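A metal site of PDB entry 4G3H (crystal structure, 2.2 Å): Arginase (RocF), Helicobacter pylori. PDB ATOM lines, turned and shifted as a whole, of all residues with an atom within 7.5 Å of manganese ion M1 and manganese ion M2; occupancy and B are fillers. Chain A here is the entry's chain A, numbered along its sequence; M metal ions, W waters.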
ATOM      1  N   GLU A  90      31.314   2.462 -26.219  1.00  0.00           N
ATOM      2  CA  GLU A  90      30.922   3.649 -25.624  1.00  0.00           C
ATOM      3  C   GLU A  90      29.655   4.245 -26.147  1.00  0.00           C
ATOM      4  O   GLU A  90      29.483   4.185 -27.208  1.00  0.00           O
ATOM      5  CB  GLU A  90      32.088   4.620 -25.491  1.00  0.00           C
ATOM      6  CG  GLU A  90      32.708   5.093 -26.648  1.00  0.00           C
ATOM      7  CD  GLU A  90      33.924   5.964 -26.356  1.00  0.00           C
ATOM      8  OE1 GLU A  90      34.955   5.570 -25.877  1.00  0.00           O
ATOM      9  OE2 GLU A  90      33.866   7.048 -26.692  1.00  0.00           O
ATOM     10  N   HIS A  91      28.758   4.701 -25.280  1.00  0.00           N
ATOM     11  CA  HIS A  91      27.503   5.212 -25.772  1.00  0.00           C
ATOM     12  C   HIS A  91      27.570   6.303 -26.828  1.00  0.00           C
ATOM     13  O   HIS A  91      26.677   6.415 -27.661  1.00  0.00           O
ATOM     14  CB  HIS A  91      26.608   5.676 -24.623  1.00  0.00           C
ATOM     15  CG  HIS A  91      25.213   5.138 -24.714  1.00  0.00           C
ATOM     16  ND1 HIS A  91      24.698   4.609 -25.882  1.00  0.00           N
ATOM     17  CD2 HIS A  91      24.237   5.020 -23.786  1.00  0.00           C
ATOM     18  CE1 HIS A  91      23.466   4.185 -25.663  1.00  0.00           C
ATOM     19  NE2 HIS A  91      23.161   4.423 -24.398  1.00  0.00           N
ATOM     20  N   ALA A  92      28.619   7.111 -26.819  1.00  0.00           N
ATOM     21  CA  ALA A  92      28.739   8.173 -27.812  1.00  0.00           C
ATOM     22  C   ALA A  92      28.682   7.620 -29.234  1.00  0.00           C
ATOM     23  O   ALA A  92      28.241   8.313 -30.150  1.00  0.00           O
ATOM     24  CB  ALA A  92      30.031   8.964 -27.602  1.00  0.00           C
ATOM     25  N   TYR A 114      15.645   3.290 -24.819  1.00  0.00           N
ATOM     26  CA  TYR A 114      16.929   3.708 -24.290  1.00  0.00           C
ATOM     27  C   TYR A 114      17.048   3.417 -22.798  1.00  0.00           C
ATOM     28  O   TYR A 114      16.474   4.130 -21.974  1.00  0.00           O
ATOM     29  CB  TYR A 114      17.091   5.218 -24.536  1.00  0.00           C
ATOM     30  CG  TYR A 114      18.514   5.721 -24.676  1.00  0.00           C
ATOM     31  CD1 TYR A 114      19.201   5.564 -25.877  1.00  0.00           C
ATOM     32  CD2 TYR A 114      19.151   6.365 -23.622  1.00  0.00           C
ATOM     33  CE1 TYR A 114      20.491   6.053 -26.026  1.00  0.00           C
ATOM     34  CE2 TYR A 114      20.458   6.860 -23.759  1.00  0.00           C
ATOM     35  CZ  TYR A 114      21.117   6.704 -24.978  1.00  0.00           C
ATOM     36  OH  TYR A 114      22.391   7.192 -25.153  1.00  0.00           O
ATOM     37  N   LEU A 115      17.785   2.374 -22.442  1.00  0.00           N
ATOM     38  CA  LEU A 115      17.967   1.983 -21.035  1.00  0.00           C
ATOM     39  C   LEU A 115      19.279   2.593 -20.597  1.00  0.00           C
ATOM     40  O   LEU A 115      20.343   2.191 -21.074  1.00  0.00           O
ATOM     41  CB  LEU A 115      17.991   0.464 -20.906  1.00  0.00           C
ATOM     42  CG  LEU A 115      16.637  -0.212 -21.151  1.00  0.00           C
ATOM     43  CD1 LEU A 115      16.226  -0.045 -22.609  1.00  0.00           C
ATOM     44  CD2 LEU A 115      16.737  -1.702 -20.786  1.00  0.00           C
ATOM     45  N   ASP A 116      19.208   3.533 -19.657  1.00  0.00           N
ATOM     46  CA  ASP A 116      20.411   4.253 -19.259  1.00  0.00           C
ATOM     47  C   ASP A 116      20.175   5.049 -17.976  1.00  0.00           C
ATOM     48  O   ASP A 116      19.042   5.404 -17.656  1.00  0.00           O
ATOM     49  CB  ASP A 116      20.749   5.225 -20.400  1.00  0.00           C
ATOM     50  CG  ASP A 116      22.163   5.737 -20.369  1.00  0.00           C
ATOM     51  OD1 ASP A 116      22.691   6.090 -19.289  1.00  0.00           O
ATOM     52  OD2 ASP A 116      22.752   5.811 -21.453  1.00  0.00           O
ATOM     53  N   ALA A 117      21.250   5.312 -17.240  1.00  0.00           N
ATOM     54  CA  ALA A 117      21.133   6.105 -16.020  1.00  0.00           C
ATOM     55  C   ALA A 117      21.111   7.565 -16.457  1.00  0.00           C
ATOM     56  O   ALA A 117      20.699   8.436 -15.691  1.00  0.00           O
ATOM     57  CB  ALA A 117      22.332   5.838 -15.105  1.00  0.00           C
ATOM     58  N   HIS A 118      21.555   7.824 -17.689  1.00  0.00           N
ATOM     59  CA  HIS A 118      21.621   9.175 -18.239  1.00  0.00           C
ATOM     60  C   HIS A 118      20.743   9.400 -19.475  1.00  0.00           C
ATOM     61  O   HIS A 118      20.366   8.456 -20.167  1.00  0.00           O
ATOM     62  CB  HIS A 118      23.066   9.515 -18.626  1.00  0.00           C
ATOM     63  CG  HIS A 118      24.079   9.137 -17.592  1.00  0.00           C
ATOM     64  ND1 HIS A 118      24.715   7.911 -17.583  1.00  0.00           N
ATOM     65  CD2 HIS A 118      24.524   9.801 -16.489  1.00  0.00           C
ATOM     66  CE1 HIS A 118      25.512   7.837 -16.523  1.00  0.00           C
ATOM     67  NE2 HIS A 118      25.413   8.970 -15.853  1.00  0.00           N
ATOM     68  N   ALA A 119      20.424  10.667 -19.732  1.00  0.00           N
ATOM     69  CA  ALA A 119      19.601  11.035 -20.875  1.00  0.00           C
ATOM     70  C   ALA A 119      20.458  11.200 -22.130  1.00  0.00           C
ATOM     71  O   ALA A 119      19.969  11.083 -23.262  1.00  0.00           O
ATOM     72  CB  ALA A 119      18.855  12.347 -20.579  1.00  0.00           C
ATOM     73  N   ASP A 120      21.753  11.472 -21.936  1.00  0.00           N
ATOM     74  CA  ASP A 120      22.684  11.639 -23.048  1.00  0.00           C
ATOM     75  C   ASP A 120      22.232  12.659 -24.093  1.00  0.00           C
ATOM     76  O   ASP A 120      22.466  12.471 -25.291  1.00  0.00           O
ATOM     77  CB  ASP A 120      22.947  10.298 -23.748  1.00  0.00           C
ATOM     78  CG  ASP A 120      23.711   9.308 -22.877  1.00  0.00           C
ATOM     79  OD1 ASP A 120      24.304   9.726 -21.863  1.00  0.00           O
ATOM     80  OD2 ASP A 120      23.724   8.099 -23.219  1.00  0.00           O
ATOM     81  N   ILE A 132      32.218  13.319 -18.563  1.00  0.00           N
ATOM     82  CA  ILE A 132      31.313  12.321 -17.998  1.00  0.00           C
ATOM     83  C   ILE A 132      30.623  11.508 -19.085  1.00  0.00           C
ATOM     84  O   ILE A 132      30.994  10.368 -19.348  1.00  0.00           O
ATOM     85  CB  ILE A 132      30.252  12.986 -17.101  1.00  0.00           C
ATOM     86  CG1 ILE A 132      30.928  13.642 -15.895  1.00  0.00           C
ATOM     87  CG2 ILE A 132      29.235  11.938 -16.641  1.00  0.00           C
ATOM     88  CD1 ILE A 132      29.963  14.326 -14.942  1.00  0.00           C
ATOM     89  N   HIS A 133      29.598  12.092 -19.714  1.00  0.00           N
ATOM     90  CA  HIS A 133      28.872  11.396 -20.769  1.00  0.00           C
ATOM     91  C   HIS A 133      28.688  12.264 -22.004  1.00  0.00           C
ATOM     92  O   HIS A 133      28.643  13.498 -21.915  1.00  0.00           O
ATOM     93  CB  HIS A 133      27.510  10.924 -20.243  1.00  0.00           C
ATOM     94  CG  HIS A 133      26.530  12.019 -19.996  1.00  0.00           C
ATOM     95  ND1 HIS A 133      25.835  12.650 -21.012  1.00  0.00           N
ATOM     96  CD2 HIS A 133      26.117  12.612 -18.846  1.00  0.00           C
ATOM     97  CE1 HIS A 133      25.045  13.578 -20.492  1.00  0.00           C
ATOM     98  NE2 HIS A 133      25.195  13.574 -19.179  1.00  0.00           N
ATOM     99  N   GLY A 134      28.589  11.628 -23.162  1.00  0.00           N
ATOM    100  CA  GLY A 134      28.410  12.338 -24.421  1.00  0.00           C
ATOM    101  C   GLY A 134      26.984  12.822 -24.664  1.00  0.00           C
ATOM    102  O   GLY A 134      26.174  12.908 -23.739  1.00  0.00           O
ATOM    103  N   PRO A 136      24.906  11.692 -27.732  1.00  0.00           N
ATOM    104  CA  PRO A 136      24.419  11.067 -28.963  1.00  0.00           C
ATOM    105  C   PRO A 136      22.951  11.381 -29.247  1.00  0.00           C
ATOM    106  O   PRO A 136      22.580  11.647 -30.390  1.00  0.00           O
ATOM    107  CB  PRO A 136      24.670   9.576 -28.730  1.00  0.00           C
ATOM    108  CG  PRO A 136      24.572   9.445 -27.246  1.00  0.00           C
ATOM    109  CD  PRO A 136      25.328  10.670 -26.763  1.00  0.00           C
ATOM    110  N   SER A 186      20.364  10.638 -13.789  1.00  0.00           N
ATOM    111  CA  SER A 186      21.478  11.576 -13.670  1.00  0.00           C
ATOM    112  C   SER A 186      21.491  12.454 -14.900  1.00  0.00           C
ATOM    113  O   SER A 186      21.914  12.021 -15.977  1.00  0.00           O
ATOM    114  CB  SER A 186      22.791  10.802 -13.528  1.00  0.00           C
ATOM    115  OG  SER A 186      23.887  11.679 -13.361  1.00  0.00           O
ATOM    116  N   SER A 232      18.701   0.418 -27.176  1.00  0.00           N
ATOM    117  CA  SER A 232      20.047   0.785 -26.755  1.00  0.00           C
ATOM    118  C   SER A 232      20.154   0.623 -25.247  1.00  0.00           C
ATOM    119  O   SER A 232      19.484   1.309 -24.492  1.00  0.00           O
ATOM    120  CB  SER A 232      20.352   2.222 -27.163  1.00  0.00           C
ATOM    121  OG  SER A 232      21.730   2.510 -26.986  1.00  0.00           O
ATOM    122  N   LEU A 233      21.021  -0.303 -24.821  1.00  0.00           N
ATOM    123  CA  LEU A 233      21.203  -0.580 -23.404  1.00  0.00           C
ATOM    124  C   LEU A 233      22.555  -0.172 -22.859  1.00  0.00           C
ATOM    125  O   LEU A 233      23.595  -0.671 -23.307  1.00  0.00           O
ATOM    126  CB  LEU A 233      20.988  -2.086 -23.136  1.00  0.00           C
ATOM    127  CG  LEU A 233      21.524  -2.627 -21.786  1.00  0.00           C
ATOM    128  CD1 LEU A 233      20.845  -1.919 -20.623  1.00  0.00           C
ATOM    129  CD2 LEU A 233      21.319  -4.128 -21.690  1.00  0.00           C
ATOM    130  N   ASP A 234      22.537   0.717 -21.868  1.00  0.00           N
ATOM    131  CA  ASP A 234      23.742   1.197 -21.195  1.00  0.00           C
ATOM    132  C   ASP A 234      23.719   0.489 -19.831  1.00  0.00           C
ATOM    133  O   ASP A 234      22.800   0.672 -19.040  1.00  0.00           O
ATOM    134  CB  ASP A 234      23.671   2.715 -20.987  1.00  0.00           C
ATOM    135  CG  ASP A 234      24.934   3.274 -20.339  1.00  0.00           C
ATOM    136  OD1 ASP A 234      25.588   2.572 -19.523  1.00  0.00           O
ATOM    137  OD2 ASP A 234      25.265   4.440 -20.628  1.00  0.00           O
ATOM    138  N   LEU A 235      24.745  -0.305 -19.555  1.00  0.00           N
ATOM    139  CA  LEU A 235      24.808  -1.053 -18.316  1.00  0.00           C
ATOM    140  C   LEU A 235      24.741  -0.230 -17.022  1.00  0.00           C
ATOM    141  O   LEU A 235      24.436  -0.761 -15.956  1.00  0.00           O
ATOM    142  CB  LEU A 235      26.058  -1.944 -18.310  1.00  0.00           C
ATOM    143  CG  LEU A 235      26.101  -3.017 -19.408  1.00  0.00           C
ATOM    144  CD1 LEU A 235      27.498  -3.630 -19.488  1.00  0.00           C
ATOM    145  CD2 LEU A 235      25.052  -4.094 -19.140  1.00  0.00           C
ATOM    146  N   ASP A 236      25.027   1.062 -17.106  1.00  0.00           N
ATOM    147  CA  ASP A 236      24.975   1.865 -15.892  1.00  0.00           C
ATOM    148  C   ASP A 236      23.538   2.103 -15.425  1.00  0.00           C
ATOM    149  O   ASP A 236      23.305   2.847 -14.463  1.00  0.00           O
ATOM    150  CB  ASP A 236      25.719   3.199 -16.054  1.00  0.00           C
ATOM    151  CG  ASP A 236      25.093   4.115 -17.094  1.00  0.00           C
ATOM    152  OD1 ASP A 236      23.892   3.966 -17.409  1.00  0.00           O
ATOM    153  OD2 ASP A 236      25.814   5.000 -17.589  1.00  0.00           O
ATOM    154  N   ILE A 237      22.568   1.477 -16.091  1.00  0.00           N
ATOM    155  CA  ILE A 237      21.192   1.617 -15.661  1.00  0.00           C
ATOM    156  C   ILE A 237      21.081   0.833 -14.359  1.00  0.00           C
ATOM    157  O   ILE A 237      20.239   1.108 -13.499  1.00  0.00           O
ATOM    158  CB  ILE A 237      20.194   1.058 -16.700  1.00  0.00           C
ATOM    159  CG1 ILE A 237      18.758   1.241 -16.198  1.00  0.00           C
ATOM    160  CG2 ILE A 237      20.486  -0.398 -16.978  1.00  0.00           C
ATOM    161  CD1 ILE A 237      17.669   0.873 -17.195  1.00  0.00           C
ATOM    162  N   THR A 246      31.584  -0.122 -15.068  1.00  0.00           N
ATOM    163  CA  THR A 246      31.089   0.878 -15.991  1.00  0.00           C
ATOM    164  C   THR A 246      31.712   2.225 -15.615  1.00  0.00           C
ATOM    165  O   THR A 246      31.953   2.507 -14.435  1.00  0.00           O
ATOM    166  CB  THR A 246      29.532   0.931 -15.954  1.00  0.00           C
ATOM    167  OG1 THR A 246      29.053   1.678 -17.083  1.00  0.00           O
ATOM    168  CG2 THR A 246      29.035   1.577 -14.680  1.00  0.00           C
ATOM    169  N   VAL A 248      30.600   5.511 -15.643  1.00  0.00           N
ATOM    170  CA  VAL A 248      29.880   6.514 -14.850  1.00  0.00           C
ATOM    171  C   VAL A 248      28.767   5.851 -14.051  1.00  0.00           C
ATOM    172  O   VAL A 248      27.624   5.791 -14.499  1.00  0.00           O
ATOM    173  CB  VAL A 248      29.286   7.620 -15.759  1.00  0.00           C
ATOM    174  CG1 VAL A 248      28.625   8.693 -14.910  1.00  0.00           C
ATOM    175  CG2 VAL A 248      30.389   8.224 -16.621  1.00  0.00           C
ATOM    176  N   GLU A 250      25.952   5.364 -11.257  1.00  0.00           N
ATOM    177  CA  GLU A 250      24.955   6.210 -10.629  1.00  0.00           C
ATOM    178  C   GLU A 250      24.163   5.384  -9.617  1.00  0.00           C
ATOM    179  O   GLU A 250      23.693   4.281  -9.928  1.00  0.00           O
ATOM    180  CB  GLU A 250      24.023   6.794 -11.695  1.00  0.00           C
ATOM    181  CG  GLU A 250      24.758   7.541 -12.799  1.00  0.00           C
ATOM    182  CD  GLU A 250      25.257   8.905 -12.345  1.00  0.00           C
ATOM    183  OE1 GLU A 250      25.297   9.151 -11.120  1.00  0.00           O
ATOM    184  OE2 GLU A 250      25.624   9.726 -13.219  1.00  0.00           O
ATOM    185  N   THR A 280      26.117  -1.346 -24.346  1.00  0.00           N
ATOM    186  CA  THR A 280      27.329  -0.549 -24.250  1.00  0.00           C
ATOM    187  C   THR A 280      27.776  -0.181 -22.835  1.00  0.00           C
ATOM    188  O   THR A 280      27.083  -0.468 -21.860  1.00  0.00           O
ATOM    189  CB  THR A 280      27.104   0.762 -25.041  1.00  0.00           C
ATOM    190  OG1 THR A 280      28.343   1.449 -25.245  1.00  0.00           O
ATOM    191  CG2 THR A 280      26.137   1.671 -24.268  1.00  0.00           C
ATOM    192  N   GLU A 281      28.945   0.446 -22.757  1.00  0.00           N
ATOM    193  CA  GLU A 281      29.526   0.891 -21.499  1.00  0.00           C
ATOM    194  C   GLU A 281      29.932  -0.208 -20.530  1.00  0.00           C
ATOM    195  O   GLU A 281      29.652  -0.123 -19.325  1.00  0.00           O
ATOM    196  CB  GLU A 281      28.585   1.880 -20.803  1.00  0.00           C
ATOM    197  CG  GLU A 281      28.354   3.192 -21.578  1.00  0.00           C
ATOM    198  CD  GLU A 281      29.623   4.027 -21.768  1.00  0.00           C
ATOM    199  OE1 GLU A 281      30.585   3.845 -20.989  1.00  0.00           O
ATOM    200  OE2 GLU A 281      29.664   4.864 -22.684  1.00  0.00           O
HETATM  201 MN    MN M   1      24.914   6.162 -19.098  1.00  0.00          MN
HETATM  202 MN    MN M   2      24.654   6.416 -22.003  1.00  0.00          MN
HETATM  203  O   HOH W   1      26.728   7.477 -20.671  1.00  0.00           O
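The side-chain carboxylate (OD2) of Asp 116 sits close to a ring nitrogen (NE2) of His 91, 3.3 Å away.
The side-chain carboxylate (OD1) of Asp 236 lies within hydrogen-bond range of the backbone NH (N) of Ala 117 (3.0 Å).
OH of Tyr 114 lies close to OD2 of Asp 120, 2.5 Å away.
NE2 of His 91 sits at hydrogen-bond distance from OH of Tyr 114, 3.0 Å away.
The backbone NH of His 91 sits at hydrogen-bond distance from the side-chain carboxylate of Glu 281, 2.8 Å away.
The side-chain hydroxyl (OG1) of Thr 280 lies within hydrogen-bond range of the backbone NH (N) of His 91, 3.3 Å away.
A ring nitrogen (NE2) of His 118 sits at hydrogen-bond distance from the side-chain carboxylate (OE2) of Glu 250 (2.7 Å).
The backbone NH (N) of Asp 234 lies within hydrogen-bond range of the backbone carbonyl oxygen (O) of Leu 115 (2.8 Å).
Of the 26 residues printed, 4 come within 4 Å of manganese ion M1.
The nearest printed residue that does not touch manganese ion M1 is Ala 117 (4.2 Å).
His 91 touches manganese ion M2.
Tyr 114 touches manganese ion M2 (OH to MN, 3.96 Å).
Five residues have an atom within 4 Å of manganese ion M2: His 91, Tyr 114, Asp 116, Asp 120 and Asp 234.
Manganese ion M1 is bound by the side-chain carboxylate of Asp 236 (2.1 Å), the side-chain carboxylate of Asp 116 (2.2 Å), a ring nitrogen (ND1) of His 118 (2.3 Å) and the side-chain carboxylate of Asp 234 (2.3 Å).
Slightly farther from manganese ion M1 lies water W1 (2.7 Å).
Manganese ion M2 is bound by the side-chain carboxylate (OD2) of Asp 116 (2.1 Å).
Manganese ion M2 is bound by OD2 of Asp 120.
OD2 of Asp 234 is bound to manganese ion M2 (2.5 Å).
Water W1 is bound to manganese ion M2, 2.7 Å away.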
